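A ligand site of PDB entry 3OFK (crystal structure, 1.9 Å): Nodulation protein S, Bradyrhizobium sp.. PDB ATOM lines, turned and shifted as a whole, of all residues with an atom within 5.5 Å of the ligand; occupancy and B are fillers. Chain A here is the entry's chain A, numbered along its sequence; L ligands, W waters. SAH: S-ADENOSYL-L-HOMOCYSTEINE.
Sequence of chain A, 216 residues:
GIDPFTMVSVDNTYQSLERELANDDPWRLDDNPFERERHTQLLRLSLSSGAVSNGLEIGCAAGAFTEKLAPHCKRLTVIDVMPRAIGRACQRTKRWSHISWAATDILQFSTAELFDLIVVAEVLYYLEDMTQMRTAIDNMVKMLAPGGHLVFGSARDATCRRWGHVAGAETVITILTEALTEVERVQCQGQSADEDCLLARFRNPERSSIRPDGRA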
ATOM      1  N   LEU A  17      36.502 -29.840  -2.403  1.00  0.00           N
ATOM      2  CA  LEU A  17      35.070 -29.593  -2.343  1.00  0.00           C
ATOM      3  C   LEU A  17      34.617 -29.179  -0.923  1.00  0.00           C
ATOM      4  O   LEU A  17      33.932 -28.155  -0.754  1.00  0.00           O
ATOM      5  CB  LEU A  17      34.351 -30.860  -2.807  1.00  0.00           C
ATOM      6  CG  LEU A  17      33.888 -30.943  -4.264  1.00  0.00           C
ATOM      7  CD1 LEU A  17      34.723 -30.142  -5.236  1.00  0.00           C
ATOM      8  CD2 LEU A  17      33.690 -32.385  -4.776  1.00  0.00           C
ATOM      9  N   LEU A  21      32.936 -25.681   0.322  1.00  0.00           N
ATOM     10  CA  LEU A  21      31.569 -25.745   0.886  1.00  0.00           C
ATOM     11  C   LEU A  21      31.467 -25.245   2.347  1.00  0.00           C
ATOM     12  O   LEU A  21      30.357 -25.058   2.856  1.00  0.00           O
ATOM     13  CB  LEU A  21      31.016 -27.162   0.758  1.00  0.00           C
ATOM     14  CG  LEU A  21      30.658 -27.554  -0.699  1.00  0.00           C
ATOM     15  CD1 LEU A  21      30.611 -29.032  -0.832  1.00  0.00           C
ATOM     16  CD2 LEU A  21      29.355 -26.864  -1.202  1.00  0.00           C
ATOM     17  N   TRP A  27      32.849 -20.940  -3.751  1.00  0.00           N
ATOM     18  CA  TRP A  27      33.235 -20.558  -5.127  1.00  0.00           C
ATOM     19  C   TRP A  27      32.911 -19.094  -5.482  1.00  0.00           C
ATOM     20  O   TRP A  27      32.958 -18.701  -6.659  1.00  0.00           O
ATOM     21  CB  TRP A  27      32.603 -21.512  -6.140  1.00  0.00           C
ATOM     22  CG  TRP A  27      33.208 -22.868  -6.130  1.00  0.00           C
ATOM     23  CD1 TRP A  27      34.313 -23.284  -6.834  1.00  0.00           C
ATOM     24  CD2 TRP A  27      32.748 -24.015  -5.398  1.00  0.00           C
ATOM     25  NE1 TRP A  27      34.567 -24.601  -6.570  1.00  0.00           N
ATOM     26  CE2 TRP A  27      33.617 -25.077  -5.697  1.00  0.00           C
ATOM     27  CE3 TRP A  27      31.698 -24.231  -4.506  1.00  0.00           C
ATOM     28  CZ2 TRP A  27      33.459 -26.350  -5.150  1.00  0.00           C
ATOM     29  CZ3 TRP A  27      31.515 -25.496  -3.972  1.00  0.00           C
ATOM     30  CH2 TRP A  27      32.404 -26.544  -4.303  1.00  0.00           C
ATOM     31  N   LEU A  29      30.102 -17.777  -5.747  1.00  0.00           N
ATOM     32  CA  LEU A  29      28.991 -17.779  -6.735  1.00  0.00           C
ATOM     33  C   LEU A  29      27.943 -16.689  -6.483  1.00  0.00           C
ATOM     34  O   LEU A  29      27.203 -16.292  -7.414  1.00  0.00           O
ATOM     35  CB  LEU A  29      28.307 -19.144  -6.781  1.00  0.00           C
ATOM     36  CG  LEU A  29      29.203 -20.310  -7.225  1.00  0.00           C
ATOM     37  CD1 LEU A  29      28.566 -21.651  -6.929  1.00  0.00           C
ATOM     38  CD2 LEU A  29      29.596 -20.222  -8.693  1.00  0.00           C
ATOM     39  N   ARG A  38      27.640 -15.463 -15.409  1.00  0.00           N
ATOM     40  CA  ARG A  38      27.649 -16.850 -15.869  1.00  0.00           C
ATOM     41  C   ARG A  38      26.317 -17.549 -15.623  1.00  0.00           C
ATOM     42  O   ARG A  38      25.793 -18.249 -16.503  1.00  0.00           O
ATOM     43  CB  ARG A  38      28.765 -17.653 -15.181  1.00  0.00           C
ATOM     44  CG  ARG A  38      28.933 -19.035 -15.730  1.00  0.00           C
ATOM     45  CD  ARG A  38      30.150 -19.726 -15.104  1.00  0.00           C
ATOM     46  NE  ARG A  38      30.023 -19.891 -13.658  1.00  0.00           N
ATOM     47  CZ  ARG A  38      29.269 -20.833 -13.039  1.00  0.00           C
ATOM     48  NH1 ARG A  38      28.522 -21.723 -13.702  1.00  0.00           N
ATOM     49  NH2 ARG A  38      29.267 -20.869 -11.709  1.00  0.00           N
ATOM     50  N   HIS A  39      25.805 -17.365 -14.406  1.00  0.00           N
ATOM     51  CA  HIS A  39      24.500 -17.857 -14.036  1.00  0.00           C
ATOM     52  C   HIS A  39      23.373 -17.287 -14.876  1.00  0.00           C
ATOM     53  O   HIS A  39      22.412 -17.998 -15.174  1.00  0.00           O
ATOM     54  CB  HIS A  39      24.235 -17.553 -12.563  1.00  0.00           C
ATOM     55  CG  HIS A  39      24.828 -18.543 -11.626  1.00  0.00           C
ATOM     56  ND1 HIS A  39      24.507 -18.578 -10.291  1.00  0.00           N
ATOM     57  CD2 HIS A  39      25.671 -19.574 -11.840  1.00  0.00           C
ATOM     58  CE1 HIS A  39      25.161 -19.561  -9.704  1.00  0.00           C
ATOM     59  NE2 HIS A  39      25.863 -20.201 -10.633  1.00  0.00           N
ATOM     60  N   LEU A  42      23.760 -19.209 -18.079  1.00  0.00           N
ATOM     61  CA  LEU A  42      23.308 -20.575 -17.794  1.00  0.00           C
ATOM     62  C   LEU A  42      21.752 -20.656 -17.694  1.00  0.00           C
ATOM     63  O   LEU A  42      21.146 -21.541 -18.294  1.00  0.00           O
ATOM     64  CB  LEU A  42      24.005 -21.077 -16.522  1.00  0.00           C
ATOM     65  CG  LEU A  42      24.118 -22.585 -16.356  1.00  0.00           C
ATOM     66  CD1 LEU A  42      25.174 -23.149 -17.321  1.00  0.00           C
ATOM     67  CD2 LEU A  42      24.433 -22.958 -14.933  1.00  0.00           C
ATOM     68  N   GLU A  57      19.799 -31.007 -11.986  1.00  0.00           N
ATOM     69  CA  GLU A  57      20.965 -30.168 -11.805  1.00  0.00           C
ATOM     70  C   GLU A  57      22.043 -31.050 -11.214  1.00  0.00           C
ATOM     71  O   GLU A  57      21.773 -31.757 -10.215  1.00  0.00           O
ATOM     72  CB  GLU A  57      20.689 -28.990 -10.886  1.00  0.00           C
ATOM     73  CG  GLU A  57      21.917 -28.020 -10.823  1.00  0.00           C
ATOM     74  CD  GLU A  57      21.946 -27.063  -9.640  1.00  0.00           C
ATOM     75  OE1 GLU A  57      21.232 -27.266  -8.635  1.00  0.00           O
ATOM     76  OE2 GLU A  57      22.674 -26.052  -9.727  1.00  0.00           O
ATOM     77  N   ILE A  58      23.222 -31.049 -11.859  1.00  0.00           N
ATOM     78  CA  ILE A  58      24.380 -31.871 -11.430  1.00  0.00           C
ATOM     79  C   ILE A  58      25.450 -30.967 -10.838  1.00  0.00           C
ATOM     80  O   ILE A  58      26.135 -30.263 -11.595  1.00  0.00           O
ATOM     81  CB  ILE A  58      24.990 -32.666 -12.586  1.00  0.00           C
ATOM     82  CG1 ILE A  58      23.992 -33.691 -13.062  1.00  0.00           C
ATOM     83  CG2 ILE A  58      26.326 -33.381 -12.150  1.00  0.00           C
ATOM     84  CD1 ILE A  58      24.285 -34.249 -14.482  1.00  0.00           C
ATOM     85  N   GLY A  59      25.604 -31.037  -9.515  1.00  0.00           N
ATOM     86  CA  GLY A  59      26.543 -30.142  -8.795  1.00  0.00           C
ATOM     87  C   GLY A  59      25.881 -28.802  -8.418  1.00  0.00           C
ATOM     88  O   GLY A  59      25.699 -27.943  -9.274  1.00  0.00           O
ATOM     89  N   CYS A  60      25.549 -28.610  -7.150  1.00  0.00           N
ATOM     90  CA  CYS A  60      24.720 -27.480  -6.733  1.00  0.00           C
ATOM     91  C   CYS A  60      25.416 -26.479  -5.824  1.00  0.00           C
ATOM     92  O   CYS A  60      24.816 -25.430  -5.516  1.00  0.00           O
ATOM     93  CB  CYS A  60      23.466 -27.984  -5.996  1.00  0.00           C
ATOM     94  SG  CYS A  60      23.742 -29.033  -4.514  1.00  0.00           S
ATOM     95  N   ALA A  61      26.628 -26.763  -5.394  1.00  0.00           N
ATOM     96  CA  ALA A  61      27.326 -25.934  -4.386  1.00  0.00           C
ATOM     97  C   ALA A  61      26.333 -25.572  -3.297  1.00  0.00           C
ATOM     98  O   ALA A  61      25.654 -26.471  -2.789  1.00  0.00           O
ATOM     99  CB  ALA A  61      27.957 -24.685  -5.016  1.00  0.00           C
ATOM    100  N   PHE A  65      22.442 -21.419  -8.005  1.00  0.00           N
ATOM    101  CA  PHE A  65      21.781 -21.674  -9.284  1.00  0.00           C
ATOM    102  C   PHE A  65      20.499 -22.473  -9.128  1.00  0.00           C
ATOM    103  O   PHE A  65      19.514 -22.195  -9.823  1.00  0.00           O
ATOM    104  CB  PHE A  65      22.706 -22.298 -10.345  1.00  0.00           C
ATOM    105  CG  PHE A  65      22.084 -22.301 -11.713  1.00  0.00           C
ATOM    106  CD1 PHE A  65      22.131 -21.148 -12.495  1.00  0.00           C
ATOM    107  CD2 PHE A  65      21.401 -23.392 -12.188  1.00  0.00           C
ATOM    108  CE1 PHE A  65      21.521 -21.092 -13.740  1.00  0.00           C
ATOM    109  CE2 PHE A  65      20.814 -23.368 -13.433  1.00  0.00           C
ATOM    110  CZ  PHE A  65      20.873 -22.182 -14.219  1.00  0.00           C
ATOM    111  N   ILE A  79      21.680 -33.475  -7.828  1.00  0.00           N
ATOM    112  CA  ILE A  79      22.630 -34.426  -7.296  1.00  0.00           C
ATOM    113  C   ILE A  79      23.903 -33.670  -6.999  1.00  0.00           C
ATOM    114  O   ILE A  79      24.184 -32.617  -7.569  1.00  0.00           O
ATOM    115  CB  ILE A  79      22.865 -35.684  -8.175  1.00  0.00           C
ATOM    116  CG1 ILE A  79      23.603 -35.378  -9.483  1.00  0.00           C
ATOM    117  CG2 ILE A  79      21.494 -36.363  -8.511  1.00  0.00           C
ATOM    118  CD1 ILE A  79      24.420 -36.541 -10.011  1.00  0.00           C
ATOM    119  N   ASP A  80      24.615 -34.174  -6.021  1.00  0.00           N
ATOM    120  CA  ASP A  80      25.889 -33.666  -5.647  1.00  0.00           C
ATOM    121  C   ASP A  80      26.648 -34.733  -4.857  1.00  0.00           C
ATOM    122  O   ASP A  80      26.093 -35.440  -4.021  1.00  0.00           O
ATOM    123  CB  ASP A  80      25.749 -32.412  -4.798  1.00  0.00           C
ATOM    124  CG  ASP A  80      27.004 -31.571  -4.827  1.00  0.00           C
ATOM    125  OD1 ASP A  80      28.068 -32.014  -4.283  1.00  0.00           O
ATOM    126  OD2 ASP A  80      26.948 -30.519  -5.504  1.00  0.00           O
ATOM    127  N   VAL A  81      27.925 -34.846  -5.154  1.00  0.00           N
ATOM    128  CA  VAL A  81      28.754 -35.836  -4.513  1.00  0.00           C
ATOM    129  C   VAL A  81      28.992 -35.508  -3.045  1.00  0.00           C
ATOM    130  O   VAL A  81      29.330 -36.375  -2.248  1.00  0.00           O
ATOM    131  CB  VAL A  81      30.094 -35.928  -5.239  1.00  0.00           C
ATOM    132  CG1 VAL A  81      30.997 -34.750  -4.865  1.00  0.00           C
ATOM    133  CG2 VAL A  81      30.761 -37.238  -4.919  1.00  0.00           C
ATOM    134  N   MET A  82      28.785 -34.242  -2.661  1.00  0.00           N
ATOM    135  CA  MET A  82      29.005 -33.778  -1.295  1.00  0.00           C
ATOM    136  C   MET A  82      27.730 -33.600  -0.475  1.00  0.00           C
ATOM    137  O   MET A  82      26.966 -32.673  -0.740  1.00  0.00           O
ATOM    138  CB  MET A  82      29.752 -32.454  -1.316  1.00  0.00           C
ATOM    139  CG  MET A  82      31.120 -32.502  -2.056  1.00  0.00           C
ATOM    140  SD  MET A  82      32.234 -33.753  -1.395  1.00  0.00           S
ATOM    141  CE  MET A  82      32.689 -33.016   0.152  1.00  0.00           C
ATOM    142  N   ALA A  85      26.854 -30.043   0.309  1.00  0.00           N
ATOM    143  CA  ALA A  85      26.254 -29.257  -0.775  1.00  0.00           C
ATOM    144  C   ALA A  85      24.713 -29.401  -0.757  1.00  0.00           C
ATOM    145  O   ALA A  85      23.983 -28.399  -0.803  1.00  0.00           O
ATOM    146  CB  ALA A  85      26.812 -29.643  -2.129  1.00  0.00           C
ATOM    147  N   THR A 104      25.198 -38.155  -4.408  1.00  0.00           N
ATOM    148  CA  THR A 104      25.832 -39.193  -5.219  1.00  0.00           C
ATOM    149  C   THR A 104      26.727 -38.533  -6.244  1.00  0.00           C
ATOM    150  O   THR A 104      26.468 -37.419  -6.691  1.00  0.00           O
ATOM    151  CB  THR A 104      24.805 -40.078  -6.002  1.00  0.00           C
ATOM    152  OG1 THR A 104      23.718 -40.420  -5.140  1.00  0.00           O
ATOM    153  CG2 THR A 104      25.432 -41.369  -6.479  1.00  0.00           C
ATOM    154  N   ASP A 105      27.727 -39.274  -6.618  1.00  0.00           N
ATOM    155  CA  ASP A 105      28.611 -38.921  -7.688  1.00  0.00           C
ATOM    156  C   ASP A 105      27.831 -39.152  -8.993  1.00  0.00           C
ATOM    157  O   ASP A 105      27.038 -40.099  -9.118  1.00  0.00           O
ATOM    158  CB  ASP A 105      29.828 -39.837  -7.594  1.00  0.00           C
ATOM    159  CG  ASP A 105      30.956 -39.402  -8.490  1.00  0.00           C
ATOM    160  OD1 ASP A 105      30.715 -38.973  -9.640  1.00  0.00           O
ATOM    161  OD2 ASP A 105      32.100 -39.501  -8.018  1.00  0.00           O
ATOM    162  N   ILE A 106      28.042 -38.290  -9.983  1.00  0.00           N
ATOM    163  CA  ILE A 106      27.366 -38.481 -11.280  1.00  0.00           C
ATOM    164  C   ILE A 106      27.752 -39.851 -11.903  1.00  0.00           C
ATOM    165  O   ILE A 106      26.946 -40.474 -12.595  1.00  0.00           O
ATOM    166  CB  ILE A 106      27.615 -37.291 -12.236  1.00  0.00           C
ATOM    167  CG1 ILE A 106      26.904 -37.509 -13.592  1.00  0.00           C
ATOM    168  CG2 ILE A 106      29.095 -37.006 -12.415  1.00  0.00           C
ATOM    169  CD1 ILE A 106      25.405 -37.747 -13.478  1.00  0.00           C
ATOM    170  N   LEU A 107      28.971 -40.317 -11.602  1.00  0.00           N
ATOM    171  CA  LEU A 107      29.455 -41.639 -12.018  1.00  0.00           C
ATOM    172  C   LEU A 107      28.639 -42.776 -11.462  1.00  0.00           C
ATOM    173  O   LEU A 107      28.611 -43.855 -12.058  1.00  0.00           O
ATOM    174  CB  LEU A 107      30.911 -41.867 -11.576  1.00  0.00           C
ATOM    175  CG  LEU A 107      32.001 -41.174 -12.403  1.00  0.00           C
ATOM    176  CD1 LEU A 107      33.343 -41.562 -11.814  1.00  0.00           C
ATOM    177  CD2 LEU A 107      31.920 -41.561 -13.875  1.00  0.00           C
ATOM    178  N   ALA A 121      27.208 -27.685 -14.939  1.00  0.00           N
ATOM    179  CA  ALA A 121      28.082 -26.504 -14.998  1.00  0.00           C
ATOM    180  C   ALA A 121      29.193 -26.575 -13.954  1.00  0.00           C
ATOM    181  O   ALA A 121      28.922 -26.773 -12.776  1.00  0.00           O
ATOM    182  CB  ALA A 121      27.229 -25.206 -14.784  1.00  0.00           C
ATOM    183  N   GLU A 122      30.451 -26.479 -14.394  1.00  0.00           N
ATOM    184  CA  GLU A 122      31.613 -26.289 -13.491  1.00  0.00           C
ATOM    185  C   GLU A 122      31.757 -27.462 -12.499  1.00  0.00           C
ATOM    186  O   GLU A 122      32.122 -27.289 -11.339  1.00  0.00           O
ATOM    187  CB  GLU A 122      31.542 -24.960 -12.756  1.00  0.00           C
ATOM    188  CG  GLU A 122      31.196 -23.725 -13.617  1.00  0.00           C
ATOM    189  CD  GLU A 122      32.218 -23.457 -14.717  1.00  0.00           C
ATOM    190  OE1 GLU A 122      33.390 -23.883 -14.578  1.00  0.00           O
ATOM    191  OE2 GLU A 122      31.802 -22.858 -15.734  1.00  0.00           O
ATOM    192  N   VAL A 123      31.496 -28.638 -13.005  1.00  0.00           N
ATOM    193  CA  VAL A 123      31.560 -29.884 -12.234  1.00  0.00           C
ATOM    194  C   VAL A 123      32.397 -30.995 -12.890  1.00  0.00           C
ATOM    195  O   VAL A 123      33.156 -31.676 -12.202  1.00  0.00           O
ATOM    196  CB  VAL A 123      30.152 -30.414 -11.907  1.00  0.00           C
ATOM    197  CG1 VAL A 123      29.361 -30.629 -13.198  1.00  0.00           C
ATOM    198  CG2 VAL A 123      30.259 -31.689 -11.160  1.00  0.00           C
ATOM    199  N   TYR A 126      36.127 -32.052 -12.115  1.00  0.00           N
ATOM    200  CA  TYR A 126      36.574 -32.690 -10.870  1.00  0.00           C
ATOM    201  C   TYR A 126      36.818 -34.188 -11.047  1.00  0.00           C
ATOM    202  O   TYR A 126      37.385 -34.837 -10.198  1.00  0.00           O
ATOM    203  CB  TYR A 126      35.570 -32.435  -9.736  1.00  0.00           C
ATOM    204  CG  TYR A 126      35.550 -30.993  -9.307  1.00  0.00           C
ATOM    205  CD1 TYR A 126      36.629 -30.431  -8.639  1.00  0.00           C
ATOM    206  CD2 TYR A 126      34.461 -30.182  -9.585  1.00  0.00           C
ATOM    207  CE1 TYR A 126      36.631 -29.085  -8.240  1.00  0.00           C
ATOM    208  CE2 TYR A 126      34.460 -28.852  -9.221  1.00  0.00           C
ATOM    209  CZ  TYR A 126      35.534 -28.317  -8.543  1.00  0.00           C
ATOM    210  OH  TYR A 126      35.484 -26.997  -8.201  1.00  0.00           O
ATOM    211  N   LEU A 127      36.397 -34.764 -12.147  1.00  0.00           N
ATOM    212  CA  LEU A 127      36.632 -36.195 -12.350  1.00  0.00           C
ATOM    213  C   LEU A 127      38.128 -36.420 -12.625  1.00  0.00           C
ATOM    214  O   LEU A 127      38.840 -35.509 -13.044  1.00  0.00           O
ATOM    215  CB  LEU A 127      35.758 -36.706 -13.486  1.00  0.00           C
ATOM    216  CG  LEU A 127      34.264 -36.679 -13.173  1.00  0.00           C
ATOM    217  CD1 LEU A 127      33.492 -36.817 -14.493  1.00  0.00           C
ATOM    218  CD2 LEU A 127      33.890 -37.775 -12.176  1.00  0.00           C
HETATM  219  N   SAH L   1      26.665 -26.076 -11.017  1.00  0.00           N
HETATM  220  CA  SAH L   1      26.822 -25.012 -10.034  1.00  0.00           C
HETATM  221  CB  SAH L   1      27.842 -25.437  -8.981  1.00  0.00           C
HETATM  222  CG  SAH L   1      29.295 -25.620  -9.377  1.00  0.00           C
HETATM  223  SD  SAH L   1      30.443 -25.913  -7.984  1.00  0.00           S
HETATM  224  C   SAH L   1      27.221 -23.661 -10.648  1.00  0.00           C
HETATM  225  O   SAH L   1      27.630 -23.573 -11.804  1.00  0.00           O
HETATM  226  OXT SAH L   1      27.135 -22.629  -9.980  1.00  0.00           O
HETATM  227  C5' SAH L   1      30.651 -27.699  -8.276  1.00  0.00           C
HETATM  228  C4' SAH L   1      29.716 -28.651  -7.559  1.00  0.00           C
HETATM  229  O4' SAH L   1      29.881 -29.947  -8.121  1.00  0.00           O
HETATM  230  C3' SAH L   1      29.971 -28.782  -6.063  1.00  0.00           C
HETATM  231  O3' SAH L   1      28.729 -28.766  -5.348  1.00  0.00           O
HETATM  232  C2' SAH L   1      30.669 -30.144  -5.949  1.00  0.00           C
HETATM  233  O2' SAH L   1      30.447 -30.753  -4.700  1.00  0.00           O
HETATM  234  C1' SAH L   1      30.003 -30.887  -7.075  1.00  0.00           C
HETATM  235  N9  SAH L   1      30.670 -32.099  -7.604  1.00  0.00           N
HETATM  236  C8  SAH L   1      32.014 -32.275  -7.825  1.00  0.00           C
HETATM  237  N7  SAH L   1      32.186 -33.504  -8.365  1.00  0.00           N
HETATM  238  C5  SAH L   1      30.986 -34.106  -8.497  1.00  0.00           C
HETATM  239  C6  SAH L   1      30.658 -35.345  -9.047  1.00  0.00           C
HETATM  240  N6  SAH L   1      31.663 -36.182  -9.450  1.00  0.00           N
HETATM  241  N1  SAH L   1      29.339 -35.711  -9.057  1.00  0.00           N
HETATM  242  C2  SAH L   1      28.370 -34.835  -8.590  1.00  0.00           C
HETATM  243  N3  SAH L   1      28.711 -33.586  -8.077  1.00  0.00           N
HETATM  244  C4  SAH L   1      30.014 -33.220  -8.051  1.00  0.00           C
HETATM  245  O   HOH W   1      33.232 -25.707  -9.836  1.00  0.00           O
HETATM  246  O   HOH W   2      24.130 -25.490 -11.823  1.00  0.00           O
HETATM  247  O   HOH W   3      25.421 -27.783 -12.824  1.00  0.00           O
HETATM  248  O   HOH W   4      34.288 -35.557  -8.480  1.00  0.00           O
HETATM  249  O   HOH W   5      25.407 -22.647  -7.956  1.00  0.00           O
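NE2 of His 39 lies within hydrogen-bond range of OXT of the ligand, at 2.8 Å.
The backbone NH (N) of Ile 106 sits at hydrogen-bond distance from a nitrogen (N1) of the ligand, at 3.0 Å.
N of the ligand is in hydrogen-bond range of O of Ala 121 (2.9 Å).
NH1 of Arg 38 is in salt-bridge range of O of the ligand, 2.8 Å away.
N6 of the ligand lies within hydrogen-bond range of OD1 of Asp 105 (3.0 Å).
N of Val 81 lies within hydrogen-bond range of N3 of the ligand, 3.3 Å away.
O3' of the ligand lies within hydrogen-bond range of N of Ala 61, at 2.9 Å.
The side-chain carboxylate (OD2) of Asp 80 sits at hydrogen-bond distance from an oxygen (O3') of the ligand (2.5 Å).
The backbone carbonyl oxygen of Gly 59 sits at hydrogen-bond distance from a nitrogen (N) of the ligand (2.7 Å).
The indole nitrogen (NE1) of Trp 27 lies within hydrogen-bond range of the side-chain hydroxyl (OH) of Tyr 126 (3.0 Å).
The side-chain sulfur (SG) of Cys 60 lies within hydrogen-bond range of the backbone carbonyl oxygen (O) of Ala 85, 3.8 Å away.
N of Gly 59 is in hydrogen-bond range of O of Ile 79, 2.9 Å away.
The backbone NH (N) of Val 81 lies within hydrogen-bond range of the backbone carbonyl oxygen (O) of Thr 104 (3.3 Å).
The side-chain carboxylate (OD2) of Asp 80 is in hydrogen-bond range of the backbone NH (N) of Cys 60, at 2.9 Å.
The backbone NH of Met 82 lies within hydrogen-bond range of the side-chain carboxylate of Asp 80.
The backbone NH of Thr 104 sits at hydrogen-bond distance from the backbone carbonyl oxygen of Asp 80, 2.9 Å away.
The backbone NH (N) of Leu 107 sits at hydrogen-bond distance from the side-chain carboxylate (OD1) of Asp 105 (2.9 Å).
Residues that only touch the ligand: Met 82, Glu 122, Leu 17, Val 123, Leu 29, Cys 60, Tyr 126, Thr 104, Trp 27, Ala 85 and Leu 127.
20 residues have an atom within 4 Å of the ligand: Leu 17, Trp 27, Leu 29, Arg 38, His 39, Gly 59, Cys 60, Ala 61, Asp 80, Val 81, Met 82, Ala 85, Thr 104, Asp 105, Ile 106, Ala 121, Glu 122, Val 123, Tyr 126 and Leu 127.
Water W5 bridges an oxygen (OXT) of the ligand (2.7 Å) and the backbone NH (N) of Phe 65 (3.2 Å).
Water W2 lies within hydrogen-bond range of the side-chain carboxylate of Glu 57 (2.6 Å) and a nitrogen (N) of the ligand (2.7 Å).
Water W3 lies within hydrogen-bond range of N of Ala 121 (2.8 Å), N of the ligand (2.8 Å) and O of Ile 58 (2.9 Å).
Water W1 lies within hydrogen-bond range of the backbone carbonyl oxygen of Glu 122, the side-chain hydroxyl of Tyr 126 and a sulfur (SD) of the ligand.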
